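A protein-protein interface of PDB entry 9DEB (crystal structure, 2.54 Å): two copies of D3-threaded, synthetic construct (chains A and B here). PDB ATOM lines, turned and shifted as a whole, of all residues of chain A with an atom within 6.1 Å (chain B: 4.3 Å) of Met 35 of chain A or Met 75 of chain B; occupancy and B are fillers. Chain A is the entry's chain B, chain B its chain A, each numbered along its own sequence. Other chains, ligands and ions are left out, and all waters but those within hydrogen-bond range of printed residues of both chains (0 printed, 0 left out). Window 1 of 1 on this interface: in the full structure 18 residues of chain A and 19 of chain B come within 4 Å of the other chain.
Among the printed residues, pairs that only touch across the chains: Lys 32 of chain A with Met 39 of chain B (3.1 Å), Lys 32 of chain A with Leu 79 of chain B (3.7 Å), Met 35 of chain A with Met 39 of chain B (3.6 Å), Met 35 of chain A with Met 75 of chain B (3.5 Å), Leu 68 of chain A with Met 75 of chain B (3.7 Å), Leu 68 of chain A with Leu 78 of chain B (3.9 Å), Leu 68 of chain A with Leu 79 of chain B (3.9 Å), Lys 71 of chain A with Glu 74 of chain B (3.9 Å), Lys 71 of chain A with Met 75 of chain B (3.3 Å), Lys 71 of chain A with Leu 78 of chain B (3.8 Å), Ala 72 of chain A with Met 75 of chain B (3.5 Å), Met 75 of chain A with Ala 72 of chain B (3.6 Å) and Met 75 of chain A with Met 75 of chain B (3.6 Å).
Lys 71 of chain A touches Met 75 of chain B, but with the chains exchanged Met 75 of chain A does not touch Lys 71 of chain B (4.01 Å). Ala 72 of chain A touches Met 75 of chain B, and with the chains exchanged Met 75 of chain A touches Ala 72 of chain B. Met 75 of chain B touches its own counterpart, Met 75 of chain A. Positions printed for both chains: 39, 71, 72, 73, 75 and 76.
Of the printed residues of chain B, Lys 32 of chain A touches Met 39 and Leu 79. Of chain B, only Met 39 (3.6 Å) and Met 75 (3.5 Å) come within 4 Å of Met 35 of chain A. Ala 36 of chain A touches none of the printed residues of chain B. Printed residues of chain B within 4 Å of Leu 68 of chain A: Met 75, Leu 78 and Leu 79. Of the printed residues of chain B, Lys 71 of chain A touches Glu 74, Met 75 and Leu 78. Of the printed residues of chain A, Met 75 of chain B touches Met 35, Leu 68, Lys 71, Ala 72 and Met 75. Of the printed residues of chain A, Leu 78 of chain B touches Leu 68 and Lys 71. The nearest printed residue of chain B that does not touch Met 35 of chain A is Lys 71 of chain B (7.4 Å). The nearest residue of chain A that does not touch Met 75 of chain B is Ala 73 of chain A (5.8 Å).
Of the 18 printed residues of chain A, 6 touch a printed residue of chain B. Printed residues of chain B that touch a printed residue of chain A: Met 39, Ala 72, Glu 74, Met 75, Leu 78 and Leu 79. Hydrophobic or aromatic side chains of chain B that line the printed part of chain A: Met 39, Met 75, Leu 78 and Leu 79.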
ATOM      1  N   LEU A  30     -25.334  22.742 -16.584  1.00  0.00           N
ATOM      2  CA  LEU A  30     -26.704  23.180 -16.352  1.00  0.00           C
ATOM      3  C   LEU A  30     -27.236  24.001 -17.519  1.00  0.00           C
ATOM      4  O   LEU A  30     -28.430  23.930 -17.830  1.00  0.00           O
ATOM      5  CB  LEU A  30     -26.793  23.975 -15.049  1.00  0.00           C
ATOM      6  CG  LEU A  30     -26.413  23.208 -13.780  1.00  0.00           C
ATOM      7  CD1 LEU A  30     -26.924  23.928 -12.545  1.00  0.00           C
ATOM      8  CD2 LEU A  30     -26.929  21.778 -13.822  1.00  0.00           C
ATOM      9  N   ILE A  31     -26.373  24.777 -18.179  1.00  0.00           N
ATOM     10  CA  ILE A  31     -26.805  25.513 -19.362  1.00  0.00           C
ATOM     11  C   ILE A  31     -27.034  24.556 -20.524  1.00  0.00           C
ATOM     12  O   ILE A  31     -27.957  24.741 -21.326  1.00  0.00           O
ATOM     13  CB  ILE A  31     -25.781  26.606 -19.712  1.00  0.00           C
ATOM     14  CG1 ILE A  31     -25.598  27.543 -18.520  1.00  0.00           C
ATOM     15  CG2 ILE A  31     -26.227  27.388 -20.938  1.00  0.00           C
ATOM     16  CD1 ILE A  31     -24.725  28.723 -18.818  1.00  0.00           C
ATOM     17  N   LYS A  32     -26.206  23.515 -20.627  1.00  0.00           N
ATOM     18  CA  LYS A  32     -26.479  22.448 -21.582  1.00  0.00           C
ATOM     19  C   LYS A  32     -27.807  21.767 -21.269  1.00  0.00           C
ATOM     20  O   LYS A  32     -28.549  21.385 -22.182  1.00  0.00           O
ATOM     21  CB  LYS A  32     -25.330  21.437 -21.577  1.00  0.00           C
ATOM     22  CG  LYS A  32     -23.987  22.017 -22.022  1.00  0.00           C
ATOM     23  CD  LYS A  32     -22.839  21.033 -21.810  1.00  0.00           C
ATOM     24  CE  LYS A  32     -22.863  19.904 -22.829  1.00  0.00           C
ATOM     25  NZ  LYS A  32     -21.934  18.795 -22.472  1.00  0.00           N
ATOM     26  N   GLN A  33     -28.130  21.623 -19.981  1.00  0.00           N
ATOM     27  CA  GLN A  33     -29.424  21.070 -19.593  1.00  0.00           C
ATOM     28  C   GLN A  33     -30.548  22.068 -19.843  1.00  0.00           C
ATOM     29  O   GLN A  33     -31.607  21.701 -20.366  1.00  0.00           O
ATOM     30  CB  GLN A  33     -29.397  20.655 -18.121  1.00  0.00           C
ATOM     31  CG  GLN A  33     -28.542  19.433 -17.825  1.00  0.00           C
ATOM     32  CD  GLN A  33     -29.207  18.140 -18.249  1.00  0.00           C
ATOM     33  OE1 GLN A  33     -30.433  18.030 -18.246  1.00  0.00           O
ATOM     34  NE2 GLN A  33     -28.400  17.153 -18.623  1.00  0.00           N
ATOM     35  N   PHE A  34     -30.339  23.334 -19.468  1.00  0.00           N
ATOM     36  CA  PHE A  34     -31.368  24.351 -19.659  1.00  0.00           C
ATOM     37  C   PHE A  34     -31.717  24.511 -21.131  1.00  0.00           C
ATOM     38  O   PHE A  34     -32.892  24.483 -21.512  1.00  0.00           O
ATOM     39  CB  PHE A  34     -30.900  25.685 -19.075  1.00  0.00           C
ATOM     40  CG  PHE A  34     -31.738  26.858 -19.502  1.00  0.00           C
ATOM     41  CD1 PHE A  34     -32.949  27.115 -18.889  1.00  0.00           C
ATOM     42  CD2 PHE A  34     -31.313  27.702 -20.515  1.00  0.00           C
ATOM     43  CE1 PHE A  34     -33.727  28.190 -19.278  1.00  0.00           C
ATOM     44  CE2 PHE A  34     -32.087  28.778 -20.910  1.00  0.00           C
ATOM     45  CZ  PHE A  34     -33.294  29.023 -20.288  1.00  0.00           C
ATOM     46  N   MET A  35     -30.699  24.682 -21.975  1.00  0.00           N
ATOM     47  CA  MET A  35     -30.935  24.914 -23.393  1.00  0.00           C
ATOM     48  C   MET A  35     -31.600  23.717 -24.053  1.00  0.00           C
ATOM     49  O   MET A  35     -32.456  23.879 -24.932  1.00  0.00           O
ATOM     50  CB  MET A  35     -29.614  25.246 -24.080  1.00  0.00           C
ATOM     51  CG  MET A  35     -29.107  26.621 -23.728  1.00  0.00           C
ATOM     52  SD  MET A  35     -30.125  27.876 -24.527  1.00  0.00           S
ATOM     53  CE  MET A  35     -29.468  27.842 -26.186  1.00  0.00           C
ATOM     54  N   ALA A  36     -31.217  22.504 -23.647  1.00  0.00           N
ATOM     55  CA  ALA A  36     -31.854  21.310 -24.191  1.00  0.00           C
ATOM     56  C   ALA A  36     -33.344  21.294 -23.882  1.00  0.00           C
ATOM     57  O   ALA A  36     -34.152  20.851 -24.707  1.00  0.00           O
ATOM     58  CB  ALA A  36     -31.178  20.057 -23.638  1.00  0.00           C
ATOM     59  N   GLU A  37     -33.730  21.772 -22.698  1.00  0.00           N
ATOM     60  CA  GLU A  37     -35.145  21.826 -22.349  1.00  0.00           C
ATOM     61  C   GLU A  37     -35.816  23.063 -22.932  1.00  0.00           C
ATOM     62  O   GLU A  37     -36.942  22.982 -23.436  1.00  0.00           O
ATOM     63  CB  GLU A  37     -35.310  21.786 -20.831  1.00  0.00           C
ATOM     64  CG  GLU A  37     -34.701  20.560 -20.177  1.00  0.00           C
ATOM     65  CD  GLU A  37     -35.403  19.274 -20.575  1.00  0.00           C
ATOM     66  OE1 GLU A  37     -36.572  19.344 -21.010  1.00  0.00           O
ATOM     67  OE2 GLU A  37     -34.788  18.194 -20.453  1.00  0.00           O
ATOM     68  N   ALA A  38     -35.137  24.212 -22.888  1.00  0.00           N
ATOM     69  CA  ALA A  38     -35.692  25.429 -23.464  1.00  0.00           C
ATOM     70  C   ALA A  38     -35.847  25.343 -24.978  1.00  0.00           C
ATOM     71  O   ALA A  38     -36.549  26.176 -25.559  1.00  0.00           O
ATOM     72  CB  ALA A  38     -34.818  26.629 -23.091  1.00  0.00           C
ATOM     73  N   MET A  39     -35.222  24.361 -25.625  1.00  0.00           N
ATOM     74  CA  MET A  39     -35.336  24.162 -27.063  1.00  0.00           C
ATOM     75  C   MET A  39     -36.519  23.300 -27.465  1.00  0.00           C
ATOM     76  O   MET A  39     -36.607  22.883 -28.625  1.00  0.00           O
ATOM     77  CB  MET A  39     -34.068  23.526 -27.598  1.00  0.00           C
ATOM     78  CG  MET A  39     -33.735  24.012 -28.959  1.00  0.00           C
ATOM     79  SD  MET A  39     -33.416  25.798 -29.041  1.00  0.00           S
ATOM     80  CE  MET A  39     -32.667  26.148 -27.433  1.00  0.00           C
ATOM     81  N   LYS A  40     -37.406  22.990 -26.534  1.00  0.00           N
ATOM     82  CA  LYS A  40     -38.636  22.283 -26.852  1.00  0.00           C
ATOM     83  C   LYS A  40     -39.826  23.001 -26.230  1.00  0.00           C
ATOM     84  O   LYS A  40     -40.833  22.376 -25.892  1.00  0.00           O
ATOM     85  CB  LYS A  40     -38.563  20.827 -26.392  1.00  0.00           C
ATOM     86  CG  LYS A  40     -37.568  19.980 -27.177  1.00  0.00           C
ATOM     87  CD  LYS A  40     -37.242  18.685 -26.453  1.00  0.00           C
ATOM     88  CE  LYS A  40     -36.606  18.969 -25.107  1.00  0.00           C
ATOM     89  NZ  LYS A  40     -35.744  17.849 -24.640  1.00  0.00           N
ATOM     90  N   LEU A  54     -32.407  34.408 -17.593  1.00  0.00           N
ATOM     91  CA  LEU A  54     -31.049  33.948 -17.859  1.00  0.00           C
ATOM     92  C   LEU A  54     -30.075  35.117 -17.936  1.00  0.00           C
ATOM     93  O   LEU A  54     -28.920  34.998 -17.513  1.00  0.00           O
ATOM     94  CB  LEU A  54     -31.022  33.134 -19.150  1.00  0.00           C
ATOM     95  CG  LEU A  54     -29.713  32.464 -19.554  1.00  0.00           C
ATOM     96  CD1 LEU A  54     -29.146  31.654 -18.406  1.00  0.00           C
ATOM     97  CD2 LEU A  54     -29.966  31.580 -20.751  1.00  0.00           C
ATOM     98  N   LEU A  68     -21.674  32.480 -23.174  1.00  0.00           N
ATOM     99  CA  LEU A  68     -22.655  31.448 -23.491  1.00  0.00           C
ATOM    100  C   LEU A  68     -24.033  31.816 -22.958  1.00  0.00           C
ATOM    101  O   LEU A  68     -25.055  31.510 -23.585  1.00  0.00           O
ATOM    102  CB  LEU A  68     -22.201  30.106 -22.919  1.00  0.00           C
ATOM    103  CG  LEU A  68     -21.394  29.211 -23.857  1.00  0.00           C
ATOM    104  CD1 LEU A  68     -20.569  28.221 -23.059  1.00  0.00           C
ATOM    105  CD2 LEU A  68     -22.324  28.479 -24.812  1.00  0.00           C
ATOM    106  N   LYS A  71     -25.463  34.471 -25.484  1.00  0.00           N
ATOM    107  CA  LYS A  71     -25.881  33.802 -26.713  1.00  0.00           C
ATOM    108  C   LYS A  71     -27.121  32.949 -26.490  1.00  0.00           C
ATOM    109  O   LYS A  71     -27.936  32.786 -27.405  1.00  0.00           O
ATOM    110  CB  LYS A  71     -24.740  32.945 -27.264  1.00  0.00           C
ATOM    111  CG  LYS A  71     -24.172  33.439 -28.586  1.00  0.00           C
ATOM    112  CD  LYS A  71     -23.616  34.846 -28.444  1.00  0.00           C
ATOM    113  CE  LYS A  71     -23.355  35.483 -29.800  1.00  0.00           C
ATOM    114  NZ  LYS A  71     -23.055  36.938 -29.667  1.00  0.00           N
ATOM    115  N   ALA A  72     -27.281  32.398 -25.284  1.00  0.00           N
ATOM    116  CA  ALA A  72     -28.457  31.586 -24.991  1.00  0.00           C
ATOM    117  C   ALA A  72     -29.714  32.443 -24.903  1.00  0.00           C
ATOM    118  O   ALA A  72     -30.764  32.069 -25.436  1.00  0.00           O
ATOM    119  CB  ALA A  72     -28.242  30.803 -23.697  1.00  0.00           C
ATOM    120  N   ALA A  73     -29.627  33.595 -24.233  1.00  0.00           N
ATOM    121  CA  ALA A  73     -30.772  34.497 -24.168  1.00  0.00           C
ATOM    122  C   ALA A  73     -31.159  34.991 -25.555  1.00  0.00           C
ATOM    123  O   ALA A  73     -32.347  35.051 -25.891  1.00  0.00           O
ATOM    124  CB  ALA A  73     -30.463  35.674 -23.244  1.00  0.00           C
ATOM    125  N   MET A  75     -30.769  33.478 -28.361  1.00  0.00           N
ATOM    126  CA  MET A  75     -31.417  32.412 -29.118  1.00  0.00           C
ATOM    127  C   MET A  75     -32.882  32.272 -28.732  1.00  0.00           C
ATOM    128  O   MET A  75     -33.746  32.108 -29.603  1.00  0.00           O
ATOM    129  CB  MET A  75     -30.691  31.087 -28.903  1.00  0.00           C
ATOM    130  CG  MET A  75     -31.377  29.918 -29.579  1.00  0.00           C
ATOM    131  SD  MET A  75     -30.443  29.329 -30.996  1.00  0.00           S
ATOM    132  CE  MET A  75     -28.995  28.676 -30.165  1.00  0.00           C
ATOM    133  N   LEU A  76     -33.183  32.328 -27.432  1.00  0.00           N
ATOM    134  CA  LEU A  76     -34.567  32.188 -26.991  1.00  0.00           C
ATOM    135  C   LEU A  76     -35.421  33.348 -27.486  1.00  0.00           C
ATOM    136  O   LEU A  76     -36.597  33.162 -27.822  1.00  0.00           O
ATOM    137  CB  LEU A  76     -34.625  32.085 -25.467  1.00  0.00           C
ATOM    138  CG  LEU A  76     -33.829  30.937 -24.843  1.00  0.00           C
ATOM    139  CD1 LEU A  76     -34.107  30.842 -23.350  1.00  0.00           C
ATOM    140  CD2 LEU A  76     -34.138  29.620 -25.540  1.00  0.00           C
ATOM    141  N   MET B  39     -26.889  20.091 -27.659  1.00  0.00           N
ATOM    142  CA  MET B  39     -26.527  20.656 -26.366  1.00  0.00           C
ATOM    143  C   MET B  39     -26.045  19.611 -25.370  1.00  0.00           C
ATOM    144  O   MET B  39     -25.554  19.986 -24.302  1.00  0.00           O
ATOM    145  CB  MET B  39     -27.719  21.405 -25.765  1.00  0.00           C
ATOM    146  CG  MET B  39     -28.111  22.685 -26.492  1.00  0.00           C
ATOM    147  SD  MET B  39     -26.980  24.066 -26.219  1.00  0.00           S
ATOM    148  CE  MET B  39     -25.802  23.841 -27.559  1.00  0.00           C
ATOM    149  N   LYS B  71     -27.161  31.873 -35.218  1.00  0.00           N
ATOM    150  CA  LYS B  71     -26.975  31.909 -33.771  1.00  0.00           C
ATOM    151  C   LYS B  71     -26.749  30.518 -33.195  1.00  0.00           C
ATOM    152  O   LYS B  71     -25.999  30.366 -32.224  1.00  0.00           O
ATOM    153  CB  LYS B  71     -28.179  32.571 -33.102  1.00  0.00           C
ATOM    154  CG  LYS B  71     -27.913  33.979 -32.597  1.00  0.00           C
ATOM    155  CD  LYS B  71     -27.556  34.924 -33.731  1.00  0.00           C
ATOM    156  CE  LYS B  71     -27.272  36.322 -33.205  1.00  0.00           C
ATOM    157  NZ  LYS B  71     -26.921  37.274 -34.296  1.00  0.00           N
ATOM    158  N   ALA B  72     -27.382  29.496 -33.775  1.00  0.00           N
ATOM    159  CA  ALA B  72     -27.198  28.136 -33.278  1.00  0.00           C
ATOM    160  C   ALA B  72     -25.787  27.633 -33.554  1.00  0.00           C
ATOM    161  O   ALA B  72     -25.190  26.952 -32.712  1.00  0.00           O
ATOM    162  CB  ALA B  72     -28.235  27.204 -33.903  1.00  0.00           C
ATOM    163  N   ALA B  73     -25.239  27.954 -34.728  1.00  0.00           N
ATOM    164  CA  ALA B  73     -23.870  27.552 -35.034  1.00  0.00           C
ATOM    165  C   ALA B  73     -22.871  28.272 -34.137  1.00  0.00           C
ATOM    166  O   ALA B  73     -21.891  27.670 -33.682  1.00  0.00           O
ATOM    167  CB  ALA B  73     -23.562  27.818 -36.506  1.00  0.00           C
ATOM    168  N   GLU B  74     -23.105  29.560 -33.869  1.00  0.00           N
ATOM    169  CA  GLU B  74     -22.230  30.296 -32.963  1.00  0.00           C
ATOM    170  C   GLU B  74     -22.294  29.737 -31.548  1.00  0.00           C
ATOM    171  O   GLU B  74     -21.304  29.805 -30.809  1.00  0.00           O
ATOM    172  CB  GLU B  74     -22.592  31.782 -32.977  1.00  0.00           C
ATOM    173  CG  GLU B  74     -22.104  32.513 -34.221  1.00  0.00           C
ATOM    174  CD  GLU B  74     -22.719  33.891 -34.382  1.00  0.00           C
ATOM    175  OE1 GLU B  74     -23.504  34.307 -33.504  1.00  0.00           O
ATOM    176  OE2 GLU B  74     -22.416  34.556 -35.397  1.00  0.00           O
ATOM    177  N   MET B  75     -23.441  29.176 -31.156  1.00  0.00           N
ATOM    178  CA  MET B  75     -23.545  28.545 -29.845  1.00  0.00           C
ATOM    179  C   MET B  75     -22.713  27.271 -29.777  1.00  0.00           C
ATOM    180  O   MET B  75     -22.033  27.018 -28.776  1.00  0.00           O
ATOM    181  CB  MET B  75     -25.006  28.240 -29.522  1.00  0.00           C
ATOM    182  CG  MET B  75     -25.215  27.591 -28.162  1.00  0.00           C
ATOM    183  SD  MET B  75     -25.389  28.812 -26.853  1.00  0.00           S
ATOM    184  CE  MET B  75     -26.785  29.738 -27.484  1.00  0.00           C
ATOM    185  N   LEU B  76     -22.756  26.455 -30.834  1.00  0.00           N
ATOM    186  CA  LEU B  76     -22.011  25.201 -30.832  1.00  0.00           C
ATOM    187  C   LEU B  76     -20.509  25.449 -30.757  1.00  0.00           C
ATOM    188  O   LEU B  76     -19.784  24.713 -30.078  1.00  0.00           O
ATOM    189  CB  LEU B  76     -22.362  24.380 -32.072  1.00  0.00           C
ATOM    190  CG  LEU B  76     -23.823  23.938 -32.187  1.00  0.00           C
ATOM    191  CD1 LEU B  76     -24.046  23.139 -33.461  1.00  0.00           C
ATOM    192  CD2 LEU B  76     -24.238  23.133 -30.965  1.00  0.00           C
ATOM    193  N   LYS B  77     -20.022  26.483 -31.446  1.00  0.00           N
ATOM    194  CA  LYS B  77     -18.610  26.835 -31.334  1.00  0.00           C
ATOM    195  C   LYS B  77     -18.276  27.308 -29.925  1.00  0.00           C
ATOM    196  O   LYS B  77     -17.258  26.900 -29.354  1.00  0.00           O
ATOM    197  CB  LYS B  77     -18.253  27.910 -32.359  1.00  0.00           C
ATOM    198  CG  LYS B  77     -18.517  27.520 -33.801  1.00  0.00           C
ATOM    199  CD  LYS B  77     -18.386  28.729 -34.709  1.00  0.00           C
ATOM    200  CE  LYS B  77     -18.663  28.376 -36.156  1.00  0.00           C
ATOM    201  NZ  LYS B  77     -18.680  29.594 -37.012  1.00  0.00           N
ATOM    202  N   LEU B  78     -19.125  28.161 -29.350  1.00  0.00           N
ATOM    203  CA  LEU B  78     -18.899  28.633 -27.988  1.00  0.00           C
ATOM    204  C   LEU B  78     -18.965  27.489 -26.987  1.00  0.00           C
ATOM    205  O   LEU B  78     -18.190  27.455 -26.023  1.00  0.00           O
ATOM    206  CB  LEU B  78     -19.914  29.718 -27.634  1.00  0.00           C
ATOM    207  CG  LEU B  78     -19.495  31.166 -27.888  1.00  0.00           C
ATOM    208  CD1 LEU B  78     -18.704  31.292 -29.180  1.00  0.00           C
ATOM    209  CD2 LEU B  78     -20.726  32.054 -27.931  1.00  0.00           C
ATOM    210  N   LEU B  79     -19.889  26.547 -27.191  1.00  0.00           N
ATOM    211  CA  LEU B  79     -19.920  25.358 -26.345  1.00  0.00           C
ATOM    212  C   LEU B  79     -18.658  24.526 -26.542  1.00  0.00           C
ATOM    213  O   LEU B  79     -18.071  24.032 -25.573  1.00  0.00           O
ATOM    214  CB  LEU B  79     -21.171  24.530 -26.651  1.00  0.00           C
ATOM    215  CG  LEU B  79     -21.724  23.545 -25.609  1.00  0.00           C
ATOM    216  CD1 LEU B  79     -20.797  22.355 -25.345  1.00  0.00           C
ATOM    217  CD2 LEU B  79     -22.060  24.264 -24.311  1.00  0.00           C
